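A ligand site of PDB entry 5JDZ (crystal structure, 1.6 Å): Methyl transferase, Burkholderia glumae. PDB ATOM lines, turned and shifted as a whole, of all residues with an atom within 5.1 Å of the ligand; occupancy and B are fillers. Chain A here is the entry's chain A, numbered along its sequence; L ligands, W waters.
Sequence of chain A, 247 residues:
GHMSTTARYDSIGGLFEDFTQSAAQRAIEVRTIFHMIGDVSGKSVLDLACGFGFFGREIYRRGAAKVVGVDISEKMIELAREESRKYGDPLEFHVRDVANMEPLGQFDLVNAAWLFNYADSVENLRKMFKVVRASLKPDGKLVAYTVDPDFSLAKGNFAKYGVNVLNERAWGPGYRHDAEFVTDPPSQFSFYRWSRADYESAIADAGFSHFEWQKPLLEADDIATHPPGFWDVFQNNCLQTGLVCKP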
ATOM      1  N   TYR A   9     -13.865  -4.363 -28.286  1.00  0.00           N
ATOM      2  CA  TYR A   9     -14.510  -4.985 -27.140  1.00  0.00           C
ATOM      3  C   TYR A   9     -15.596  -5.974 -27.570  1.00  0.00           C
ATOM      4  O   TYR A   9     -16.319  -6.520 -26.734  1.00  0.00           O
ATOM      5  CB  TYR A   9     -15.111  -3.924 -26.212  1.00  0.00           C
ATOM      6  CG  TYR A   9     -14.197  -3.491 -25.082  1.00  0.00           C
ATOM      7  CD1 TYR A   9     -14.470  -3.835 -23.761  1.00  0.00           C
ATOM      8  CD2 TYR A   9     -13.051  -2.742 -25.340  1.00  0.00           C
ATOM      9  CE1 TYR A   9     -13.644  -3.446 -22.732  1.00  0.00           C
ATOM     10  CE2 TYR A   9     -12.218  -2.340 -24.308  1.00  0.00           C
ATOM     11  CZ  TYR A   9     -12.517  -2.699 -23.001  1.00  0.00           C
ATOM     12  OH  TYR A   9     -11.684  -2.295 -21.980  1.00  0.00           O
ATOM     13  N   PHE A  16     -15.769  -8.319 -19.389  1.00  0.00           N
ATOM     14  CA  PHE A  16     -15.501  -7.048 -18.722  1.00  0.00           C
ATOM     15  C   PHE A  16     -16.264  -6.931 -17.415  1.00  0.00           C
ATOM     16  O   PHE A  16     -15.769  -6.307 -16.467  1.00  0.00           O
ATOM     17  CB  PHE A  16     -15.830  -5.875 -19.645  1.00  0.00           C
ATOM     18  CG  PHE A  16     -15.673  -4.537 -18.991  1.00  0.00           C
ATOM     19  CD1 PHE A  16     -14.399  -4.049 -18.698  1.00  0.00           C
ATOM     20  CD2 PHE A  16     -16.774  -3.775 -18.643  1.00  0.00           C
ATOM     21  CE1 PHE A  16     -14.241  -2.819 -18.080  1.00  0.00           C
ATOM     22  CE2 PHE A  16     -16.616  -2.545 -18.026  1.00  0.00           C
ATOM     23  CZ  PHE A  16     -15.350  -2.065 -17.754  1.00  0.00           C
ATOM     24  N   THR A  20     -15.151  -6.201 -13.466  1.00  0.00           N
ATOM     25  CA  THR A  20     -15.682  -5.201 -12.554  1.00  0.00           C
ATOM     26  C   THR A  20     -16.090  -5.814 -11.214  1.00  0.00           C
ATOM     27  O   THR A  20     -16.108  -5.111 -10.188  1.00  0.00           O
ATOM     28  CB  THR A  20     -16.878  -4.479 -13.192  1.00  0.00           C
ATOM     29  OG1 THR A  20     -17.911  -5.421 -13.487  1.00  0.00           O
ATOM     30  CG2 THR A  20     -16.450  -3.797 -14.484  1.00  0.00           C
ATOM     31  N   ARG A  26     -11.657  -1.690  -8.870  1.00  0.00           N
ATOM     32  CA  ARG A  26     -12.981  -1.255  -9.318  1.00  0.00           C
ATOM     33  C   ARG A  26     -13.766  -0.534  -8.223  1.00  0.00           C
ATOM     34  O   ARG A  26     -14.469   0.446  -8.507  1.00  0.00           O
ATOM     35  CB  ARG A  26     -13.783  -2.418  -9.877  1.00  0.00           C
ATOM     36  CG  ARG A  26     -15.099  -2.003 -10.578  1.00  0.00           C
ATOM     37  CD  ARG A  26     -14.911  -1.169 -11.860  1.00  0.00           C
ATOM     38  NE  ARG A  26     -16.191  -1.032 -12.567  1.00  0.00           N
ATOM     39  CZ  ARG A  26     -16.383  -0.422 -13.732  1.00  0.00           C
ATOM     40  NH1 ARG A  26     -15.385   0.146 -14.382  1.00  0.00           N
ATOM     41  NH2 ARG A  26     -17.605  -0.377 -14.257  1.00  0.00           N
ATOM     42  N   GLU A  29     -12.462   3.021  -8.261  1.00  0.00           N
ATOM     43  CA  GLU A  29     -12.906   3.752  -9.434  1.00  0.00           C
ATOM     44  C   GLU A  29     -14.372   4.182  -9.295  1.00  0.00           C
ATOM     45  O   GLU A  29     -14.731   5.340  -9.551  1.00  0.00           O
ATOM     46  CB  GLU A  29     -12.685   2.884 -10.680  1.00  0.00           C
ATOM     47  CG  GLU A  29     -13.607   3.164 -11.842  1.00  0.00           C
ATOM     48  CD  GLU A  29     -13.402   2.183 -12.991  1.00  0.00           C
ATOM     49  OE1 GLU A  29     -12.812   1.100 -12.771  1.00  0.00           O
ATOM     50  OE2 GLU A  29     -13.824   2.492 -14.123  1.00  0.00           O
ATOM     51  N   LEU A  48     -20.759   8.023 -22.036  1.00  0.00           N
ATOM     52  CA  LEU A  48     -19.953   7.773 -23.232  1.00  0.00           C
ATOM     53  C   LEU A  48     -18.975   6.632 -22.971  1.00  0.00           C
ATOM     54  O   LEU A  48     -18.428   6.517 -21.876  1.00  0.00           O
ATOM     55  CB  LEU A  48     -19.166   9.021 -23.630  1.00  0.00           C
ATOM     56  CG  LEU A  48     -20.035  10.211 -24.046  1.00  0.00           C
ATOM     57  CD1 LEU A  48     -19.115  11.387 -24.433  1.00  0.00           C
ATOM     58  CD2 LEU A  48     -20.971   9.860 -25.187  1.00  0.00           C
ATOM     59  N   ALA A  49     -18.718   5.819 -24.008  1.00  0.00           N
ATOM     60  CA  ALA A  49     -17.973   4.560 -23.845  1.00  0.00           C
ATOM     61  C   ALA A  49     -18.627   3.685 -22.771  1.00  0.00           C
ATOM     62  O   ALA A  49     -17.970   3.169 -21.868  1.00  0.00           O
ATOM     63  CB  ALA A  49     -16.500   4.809 -23.520  1.00  0.00           C
ATOM     64  N   CYS A  50     -19.948   3.523 -22.881  1.00  0.00           N
ATOM     65  CA  CYS A  50     -20.733   3.036 -21.751  1.00  0.00           C
ATOM     66  C   CYS A  50     -20.562   1.541 -21.481  1.00  0.00           C
ATOM     67  O   CYS A  50     -20.980   1.089 -20.411  1.00  0.00           O
ATOM     68  CB  CYS A  50     -22.215   3.334 -22.004  1.00  0.00           C
ATOM     69  SG  CYS A  50     -22.952   2.504 -23.440  1.00  0.00           S
ATOM     70  N   GLY A  51     -20.002   0.778 -22.408  1.00  0.00           N
ATOM     71  CA  GLY A  51     -19.877  -0.655 -22.184  1.00  0.00           C
ATOM     72  C   GLY A  51     -21.248  -1.307 -22.104  1.00  0.00           C
ATOM     73  O   GLY A  51     -22.136  -1.027 -22.927  1.00  0.00           O
ATOM     74  N   PHE A  52     -21.437  -2.195 -21.123  1.00  0.00           N
ATOM     75  CA  PHE A  52     -22.762  -2.747 -20.876  1.00  0.00           C
ATOM     76  C   PHE A  52     -23.658  -1.796 -20.062  1.00  0.00           C
ATOM     77  O   PHE A  52     -24.783  -2.189 -19.707  1.00  0.00           O
ATOM     78  CB  PHE A  52     -22.676  -4.123 -20.194  1.00  0.00           C
ATOM     79  CG  PHE A  52     -22.065  -4.106 -18.821  1.00  0.00           C
ATOM     80  CD1 PHE A  52     -22.830  -3.833 -17.712  1.00  0.00           C
ATOM     81  CD2 PHE A  52     -20.721  -4.413 -18.650  1.00  0.00           C
ATOM     82  CE1 PHE A  52     -22.273  -3.828 -16.443  1.00  0.00           C
ATOM     83  CE2 PHE A  52     -20.145  -4.402 -17.381  1.00  0.00           C
ATOM     84  CZ  PHE A  52     -20.926  -4.110 -16.277  1.00  0.00           C
ATOM     85  N   PHE A  54     -22.803   0.131 -17.135  1.00  0.00           N
ATOM     86  CA  PHE A  54     -22.695   0.110 -15.680  1.00  0.00           C
ATOM     87  C   PHE A  54     -22.959   1.475 -15.064  1.00  0.00           C
ATOM     88  O   PHE A  54     -23.822   1.620 -14.201  1.00  0.00           O
ATOM     89  CB  PHE A  54     -21.318  -0.401 -15.251  1.00  0.00           C
ATOM     90  CG  PHE A  54     -21.127  -0.354 -13.760  1.00  0.00           C
ATOM     91  CD1 PHE A  54     -21.621  -1.380 -12.963  1.00  0.00           C
ATOM     92  CD2 PHE A  54     -20.523   0.730 -13.155  1.00  0.00           C
ATOM     93  CE1 PHE A  54     -21.475  -1.336 -11.596  1.00  0.00           C
ATOM     94  CE2 PHE A  54     -20.379   0.781 -11.776  1.00  0.00           C
ATOM     95  CZ  PHE A  54     -20.858  -0.257 -11.002  1.00  0.00           C
ATOM     96  N   PHE A  55     -22.224   2.504 -15.504  1.00  0.00           N
ATOM     97  CA  PHE A  55     -22.321   3.782 -14.820  1.00  0.00           C
ATOM     98  C   PHE A  55     -23.649   4.465 -15.104  1.00  0.00           C
ATOM     99  O   PHE A  55     -24.306   4.944 -14.184  1.00  0.00           O
ATOM    100  CB  PHE A  55     -21.137   4.677 -15.187  1.00  0.00           C
ATOM    101  CG  PHE A  55     -19.905   4.295 -14.457  1.00  0.00           C
ATOM    102  CD1 PHE A  55     -19.804   4.543 -13.101  1.00  0.00           C
ATOM    103  CD2 PHE A  55     -18.894   3.611 -15.094  1.00  0.00           C
ATOM    104  CE1 PHE A  55     -18.672   4.153 -12.412  1.00  0.00           C
ATOM    105  CE2 PHE A  55     -17.762   3.221 -14.405  1.00  0.00           C
ATOM    106  CZ  PHE A  55     -17.657   3.495 -13.063  1.00  0.00           C
ATOM    107  N   VAL A  70     -23.667   5.487 -24.985  1.00  0.00           N
ATOM    108  CA  VAL A  70     -23.050   5.415 -26.300  1.00  0.00           C
ATOM    109  C   VAL A  70     -21.799   4.554 -26.202  1.00  0.00           C
ATOM    110  O   VAL A  70     -20.984   4.747 -25.303  1.00  0.00           O
ATOM    111  CB  VAL A  70     -22.682   6.810 -26.830  1.00  0.00           C
ATOM    112  CG1 VAL A  70     -21.957   6.687 -28.159  1.00  0.00           C
ATOM    113  CG2 VAL A  70     -23.921   7.671 -26.959  1.00  0.00           C
ATOM    114  N   ASP A  71     -21.675   3.597 -27.117  1.00  0.00           N
ATOM    115  CA  ASP A  71     -20.468   2.787 -27.232  1.00  0.00           C
ATOM    116  C   ASP A  71     -20.255   2.476 -28.702  1.00  0.00           C
ATOM    117  O   ASP A  71     -21.221   2.353 -29.457  1.00  0.00           O
ATOM    118  CB  ASP A  71     -20.580   1.499 -26.402  1.00  0.00           C
ATOM    119  CG  ASP A  71     -19.225   0.865 -26.106  1.00  0.00           C
ATOM    120  OD1 ASP A  71     -18.767   0.988 -24.951  1.00  0.00           O
ATOM    121  OD2 ASP A  71     -18.636   0.258 -27.026  1.00  0.00           O
ATOM    122  N   ILE A  72     -18.988   2.364 -29.100  1.00  0.00           N
ATOM    123  CA  ILE A  72     -18.644   2.048 -30.480  1.00  0.00           C
ATOM    124  C   ILE A  72     -18.842   0.573 -30.807  1.00  0.00           C
ATOM    125  O   ILE A  72     -18.943   0.216 -31.983  1.00  0.00           O
ATOM    126  CB  ILE A  72     -17.202   2.486 -30.778  1.00  0.00           C
ATOM    127  CG1 ILE A  72     -16.945   2.624 -32.283  1.00  0.00           C
ATOM    128  CG2 ILE A  72     -16.214   1.509 -30.179  1.00  0.00           C
ATOM    129  CD1 ILE A  72     -15.564   3.141 -32.622  1.00  0.00           C
ATOM    130  N   SER A  73     -18.937  -0.284 -29.799  1.00  0.00           N
ATOM    131  CA  SER A  73     -19.046  -1.730 -30.007  1.00  0.00           C
ATOM    132  C   SER A  73     -20.503  -2.158 -30.067  1.00  0.00           C
ATOM    133  O   SER A  73     -21.262  -1.920 -29.110  1.00  0.00           O
ATOM    134  CB  SER A  73     -18.318  -2.499 -28.910  1.00  0.00           C
ATOM    135  OG  SER A  73     -18.684  -3.869 -28.950  1.00  0.00           O
ATOM    136  N   MET A  76     -21.194  -4.710 -27.116  1.00  0.00           N
ATOM    137  CA  MET A  76     -21.420  -4.097 -25.799  1.00  0.00           C
ATOM    138  C   MET A  76     -22.790  -3.440 -25.729  1.00  0.00           C
ATOM    139  O   MET A  76     -23.447  -3.473 -24.687  1.00  0.00           O
ATOM    140  CB  MET A  76     -20.326  -3.079 -25.476  1.00  0.00           C
ATOM    141  CG  MET A  76     -18.907  -3.645 -25.381  1.00  0.00           C
ATOM    142  SD  MET A  76     -18.723  -4.981 -24.187  1.00  0.00           S
ATOM    143  CE  MET A  76     -18.753  -4.068 -22.645  1.00  0.00           C
ATOM    144  N   ARG A  96     -22.130   4.333 -31.542  1.00  0.00           N
ATOM    145  CA  ARG A  96     -21.485   5.432 -32.242  1.00  0.00           C
ATOM    146  C   ARG A  96     -20.019   5.542 -31.838  1.00  0.00           C
ATOM    147  O   ARG A  96     -19.643   5.179 -30.718  1.00  0.00           O
ATOM    148  CB  ARG A  96     -22.209   6.765 -31.986  1.00  0.00           C
ATOM    149  CG  ARG A  96     -23.476   6.917 -32.824  1.00  0.00           C
ATOM    150  CD  ARG A  96     -24.310   8.137 -32.460  1.00  0.00           C
ATOM    151  NE  ARG A  96     -25.712   7.945 -32.844  1.00  0.00           N
ATOM    152  CZ  ARG A  96     -26.623   8.902 -32.801  1.00  0.00           C
ATOM    153  NH1 ARG A  96     -26.295  10.121 -32.416  1.00  0.00           N
ATOM    154  NH2 ARG A  96     -27.873   8.641 -33.163  1.00  0.00           N
ATOM    155  N   ASP A  97     -19.203   6.029 -32.762  1.00  0.00           N
ATOM    156  CA  ASP A  97     -17.827   6.408 -32.466  1.00  0.00           C
ATOM    157  C   ASP A  97     -17.852   7.818 -31.884  1.00  0.00           C
ATOM    158  O   ASP A  97     -18.204   8.768 -32.583  1.00  0.00           O
ATOM    159  CB  ASP A  97     -16.958   6.351 -33.719  1.00  0.00           C
ATOM    160  CG  ASP A  97     -15.536   6.879 -33.501  1.00  0.00           C
ATOM    161  OD1 ASP A  97     -15.129   7.149 -32.350  1.00  0.00           O
ATOM    162  OD2 ASP A  97     -14.816   7.017 -34.508  1.00  0.00           O
ATOM    163  N   VAL A  98     -17.476   7.950 -30.602  1.00  0.00           N
ATOM    164  CA  VAL A  98     -17.621   9.258 -29.961  1.00  0.00           C
ATOM    165  C   VAL A  98     -16.797  10.316 -30.673  1.00  0.00           C
ATOM    166  O   VAL A  98     -17.182  11.487 -30.710  1.00  0.00           O
ATOM    167  CB  VAL A  98     -17.265   9.157 -28.457  1.00  0.00           C
ATOM    168  CG1 VAL A  98     -17.138  10.540 -27.844  1.00  0.00           C
ATOM    169  CG2 VAL A  98     -18.333   8.379 -27.734  1.00  0.00           C
ATOM    170  N   ALA A  99     -15.657   9.943 -31.247  1.00  0.00           N
ATOM    171  CA  ALA A  99     -14.812  10.947 -31.891  1.00  0.00           C
ATOM    172  C   ALA A  99     -15.464  11.509 -33.143  1.00  0.00           C
ATOM    173  O   ALA A  99     -15.103  12.609 -33.570  1.00  0.00           O
ATOM    174  CB  ALA A  99     -13.453  10.345 -32.235  1.00  0.00           C
ATOM    175  N   ALA A 113     -16.256   7.154 -18.431  1.00  0.00           N
ATOM    176  CA  ALA A 113     -15.352   6.271 -17.704  1.00  0.00           C
ATOM    177  C   ALA A 113     -14.672   5.350 -18.713  1.00  0.00           C
ATOM    178  O   ALA A 113     -15.302   4.418 -19.229  1.00  0.00           O
ATOM    179  CB  ALA A 113     -16.111   5.476 -16.640  1.00  0.00           C
ATOM    180  N   TRP A 114     -13.385   5.624 -18.966  1.00  0.00           N
ATOM    181  CA  TRP A 114     -12.531   4.845 -19.871  1.00  0.00           C
ATOM    182  C   TRP A 114     -12.912   5.067 -21.334  1.00  0.00           C
ATOM    183  O   TRP A 114     -12.999   4.139 -22.136  1.00  0.00           O
ATOM    184  CB  TRP A 114     -12.550   3.351 -19.525  1.00  0.00           C
ATOM    185  CG  TRP A 114     -12.137   3.101 -18.131  1.00  0.00           C
ATOM    186  CD1 TRP A 114     -12.915   2.577 -17.144  1.00  0.00           C
ATOM    187  CD2 TRP A 114     -10.862   3.379 -17.549  1.00  0.00           C
ATOM    188  NE1 TRP A 114     -12.191   2.484 -15.975  1.00  0.00           N
ATOM    189  CE2 TRP A 114     -10.931   2.968 -16.196  1.00  0.00           C
ATOM    190  CE3 TRP A 114      -9.665   3.911 -18.036  1.00  0.00           C
ATOM    191  CZ2 TRP A 114      -9.843   3.079 -15.333  1.00  0.00           C
ATOM    192  CZ3 TRP A 114      -8.598   4.026 -17.171  1.00  0.00           C
ATOM    193  CH2 TRP A 114      -8.697   3.612 -15.840  1.00  0.00           C
ATOM    194  N   LEU A 115     -13.133   6.341 -21.678  1.00  0.00           N
ATOM    195  CA  LEU A 115     -13.266   6.776 -23.062  1.00  0.00           C
ATOM    196  C   LEU A 115     -11.947   7.260 -23.645  1.00  0.00           C
ATOM    197  O   LEU A 115     -11.512   6.783 -24.706  1.00  0.00           O
ATOM    198  CB  LEU A 115     -14.293   7.911 -23.138  1.00  0.00           C
ATOM    199  CG  LEU A 115     -14.408   8.617 -24.518  1.00  0.00           C
ATOM    200  CD1 LEU A 115     -14.921   7.665 -25.587  1.00  0.00           C
ATOM    201  CD2 LEU A 115     -15.272   9.889 -24.440  1.00  0.00           C
ATOM    202  N   TYR A 118      -8.931   5.465 -25.184  1.00  0.00           N
ATOM    203  CA  TYR A 118      -9.094   4.748 -26.448  1.00  0.00           C
ATOM    204  C   TYR A 118      -8.995   5.664 -27.647  1.00  0.00           C
ATOM    205  O   TYR A 118      -9.131   5.200 -28.777  1.00  0.00           O
ATOM    206  CB  TYR A 118     -10.406   3.973 -26.451  1.00  0.00           C
ATOM    207  CG  TYR A 118     -10.330   2.870 -25.414  1.00  0.00           C
ATOM    208  CD1 TYR A 118      -9.631   1.702 -25.670  1.00  0.00           C
ATOM    209  CD2 TYR A 118     -10.881   3.050 -24.156  1.00  0.00           C
ATOM    210  CE1 TYR A 118      -9.510   0.713 -24.699  1.00  0.00           C
ATOM    211  CE2 TYR A 118     -10.758   2.052 -23.187  1.00  0.00           C
ATOM    212  CZ  TYR A 118     -10.081   0.895 -23.471  1.00  0.00           C
ATOM    213  OH  TYR A 118      -9.951  -0.086 -22.519  1.00  0.00           O
ATOM    214  N   MET A 128     -12.734  14.145 -29.466  1.00  0.00           N
ATOM    215  CA  MET A 128     -13.624  13.638 -28.422  1.00  0.00           C
ATOM    216  C   MET A 128     -14.010  14.739 -27.446  1.00  0.00           C
ATOM    217  O   MET A 128     -15.182  14.852 -27.069  1.00  0.00           O
ATOM    218  CB  MET A 128     -12.973  12.464 -27.679  1.00  0.00           C
ATOM    219  CG  MET A 128     -12.911  11.182 -28.477  1.00  0.00           C
ATOM    220  SD  MET A 128     -12.177   9.914 -27.430  1.00  0.00           S
ATOM    221  CE  MET A 128     -12.226   8.490 -28.519  1.00  0.00           C
HETATM  222  N1  LIG L   1     -17.572   2.782 -19.210  1.00  0.00           N
HETATM  223  C1  LIG L   1     -17.736   1.347 -19.012  1.00  0.00           C
HETATM  224  C2  LIG L   1     -16.883   0.502 -19.954  1.00  0.00           C
HETATM  225  C3  LIG L   1     -15.451   0.996 -20.145  1.00  0.00           C
HETATM  226  S1  LIG L   1     -14.572  -0.203 -21.101  1.00  0.00           S
HETATM  227  C4  LIG L   1     -17.422   1.034 -17.560  1.00  0.00           C
HETATM  228  O1  LIG L   1     -18.077   0.141 -16.974  1.00  0.00           O
HETATM  229  O2  LIG L   1     -16.521   1.691 -17.002  1.00  0.00           O
HETATM  230  C5  LIG L   1     -14.169   0.780 -22.515  1.00  0.00           C
HETATM  231  C6  LIG L   1     -15.334   0.888 -23.488  1.00  0.00           C
HETATM  232  O3  LIG L   1     -15.115   1.989 -24.386  1.00  0.00           O
HETATM  233  C7  LIG L   1     -15.553  -0.336 -24.371  1.00  0.00           C
HETATM  234  O4  LIG L   1     -16.903  -0.782 -24.190  1.00  0.00           O
HETATM  235  C8  LIG L   1     -15.283   0.150 -25.790  1.00  0.00           C
HETATM  236  O5  LIG L   1     -16.085  -0.480 -26.816  1.00  0.00           O
HETATM  237  C9  LIG L   1     -15.593   1.630 -25.691  1.00  0.00           C
HETATM  238  N2  LIG L   1     -14.970   2.494 -26.716  1.00  0.00           N
HETATM  239  C10 LIG L   1     -13.698   2.446 -27.150  1.00  0.00           C
HETATM  240  N3  LIG L   1     -13.466   3.427 -28.067  1.00  0.00           N
HETATM  241  C11 LIG L   1     -14.622   4.105 -28.222  1.00  0.00           C
HETATM  242  C12 LIG L   1     -15.061   5.241 -29.039  1.00  0.00           C
HETATM  243  N4  LIG L   1     -14.194   5.831 -29.887  1.00  0.00           N
HETATM  244  N5  LIG L   1     -16.347   5.659 -28.905  1.00  0.00           N
HETATM  245  C13 LIG L   1     -17.206   5.043 -28.074  1.00  0.00           C
HETATM  246  N6  LIG L   1     -16.862   3.996 -27.295  1.00  0.00           N
HETATM  247  C14 LIG L   1     -15.609   3.491 -27.337  1.00  0.00           C
HETATM  248  O   HOH W   1     -20.277  -1.192 -18.344  1.00  0.00           O
HETATM  249  O   HOH W   2     -12.171  -0.175 -28.218  1.00  0.00           O
HETATM  250  O   HOH W   3     -20.620   2.857 -18.111  1.00  0.00           O
HETATM  251  O   HOH W   4     -18.628   5.595 -19.267  1.00  0.00           O
HETATM  252  O   HOH W   5     -14.519  -1.657 -28.520  1.00  0.00           O
HETATM  253  O   HOH W   6     -11.434   5.293 -30.579  1.00  0.00           O
HETATM  254  O   HOH W   7     -11.549   2.062 -29.730  1.00  0.00           O
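Water W5 lies within hydrogen-bond range of an oxygen (O5) of the ligand (2.6 Å) and the backbone NH (N) of Tyr 9 (2.8 Å). Water W6 lies within hydrogen-bond range of N4 of the ligand and O of Tyr 118. Water W1 lies within hydrogen-bond range of O1 of the ligand (2.9 Å), N of Phe 54 (3.1 Å), O of Cys 50 (3.2 Å) and N of Phe 52 (3.2 Å). Water W4 lies within hydrogen-bond range of O of Leu 48 (2.8 Å), N of Ala 113 (3.0 Å) and N1 of the ligand (3.0 Å). Water W3 lies within hydrogen-bond range of the backbone carbonyl oxygen of Cys 50 (2.9 Å), the backbone NH of Phe 55 (3.1 Å) and a nitrogen (N1) of the ligand (3.2 Å).
The side-chain carboxylate of Asp 71 is in hydrogen-bond range of the backbone NH of Cys 50, at 3.5 Å. The backbone NH (N) of Gly 51 sits at hydrogen-bond distance from the side-chain carboxylate (OD1) of Asp 71 (2.8 Å). The backbone carbonyl oxygen of Asp 71 sits at hydrogen-bond distance from the backbone NH of Arg 96 (3.0 Å). O of Val 70 is in hydrogen-bond range of N of Ala 49. OE2 of Glu 29 is in salt-bridge range of NH1 of Arg 26 (2.8 Å). The side-chain carboxylate (OD1) of Asp 97 is in hydrogen-bond range of the backbone NH (N) of Ala 99 (3.0 Å). O of Arg 96 lies close to N of Ile 72, at 3.3 Å. The side-chain hydroxyl (OG) of Ser 73 is in hydrogen-bond range of the backbone NH (N) of Met 76.
The side-chain carboxylate of Asp 71 lies within hydrogen-bond range of an oxygen (O5) of the ligand, 2.7 Å away. The backbone carbonyl oxygen (O) of Ala 49 lies within hydrogen-bond range of a nitrogen (N1) of the ligand, 2.7 Å away. N1 of the ligand lies within hydrogen-bond range of O of Ala 113 (2.8 Å). The guanidinium group (NH2) of Arg 26 is in salt-bridge range of an oxygen (O1) of the ligand (2.8 Å). The side-chain carboxylate (OD1) of Asp 97 lies within hydrogen-bond range of a nitrogen (N4) of the ligand (2.9 Å). N5 of the ligand sits at hydrogen-bond distance from N of Val 98, 3.1 Å away. The backbone NH (N) of Ile 72 sits at hydrogen-bond distance from a nitrogen (N6) of the ligand (3.2 Å). A sulfur (S1) of the ligand lies close to the side-chain hydroxyl (OH) of Tyr 9.
Phe 16 touches the ligand. Cys 50 touches the ligand (O to C1, 3.5 Å). CA of Gly 51 touches O4 of the ligand, at 3.6 Å. CB of Phe 54 touches O1 of the ligand (3.7 Å). Phe 55 touches the ligand (CE2 to O2, 3.3 Å). Ser 73 touches the ligand. CG of Met 76 touches O4 of the ligand, at 3.7 Å. O of Arg 96 touches C13 of the ligand, at 3.6 Å. O of Trp 114 touches C5 of the ligand, at 3.6 Å. Tyr 118 touches the ligand. Met 128 touches the ligand (CE to N4, 3.6 Å). Hydrophobic or aromatic side chains that line the ligand: Tyr 9, Phe 16, Ala 49, Phe 54, Phe 55, Ile 72, Met 76, Val 98, Ala 113, Trp 114, Tyr 118 and Met 128. 19 residues have an atom within 4 Å of the ligand: Tyr 9, Phe 16, Arg 26, Ala 49, Cys 50, Gly 51, Phe 54, Phe 55, Asp 71, Ile 72, Ser 73, Met 76, Arg 96, Asp 97, Val 98, Ala 113, Trp 114, Tyr 118 and Met 128. The nearest printed residue that does not touch the ligand is Glu 29 (4.03 Å).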
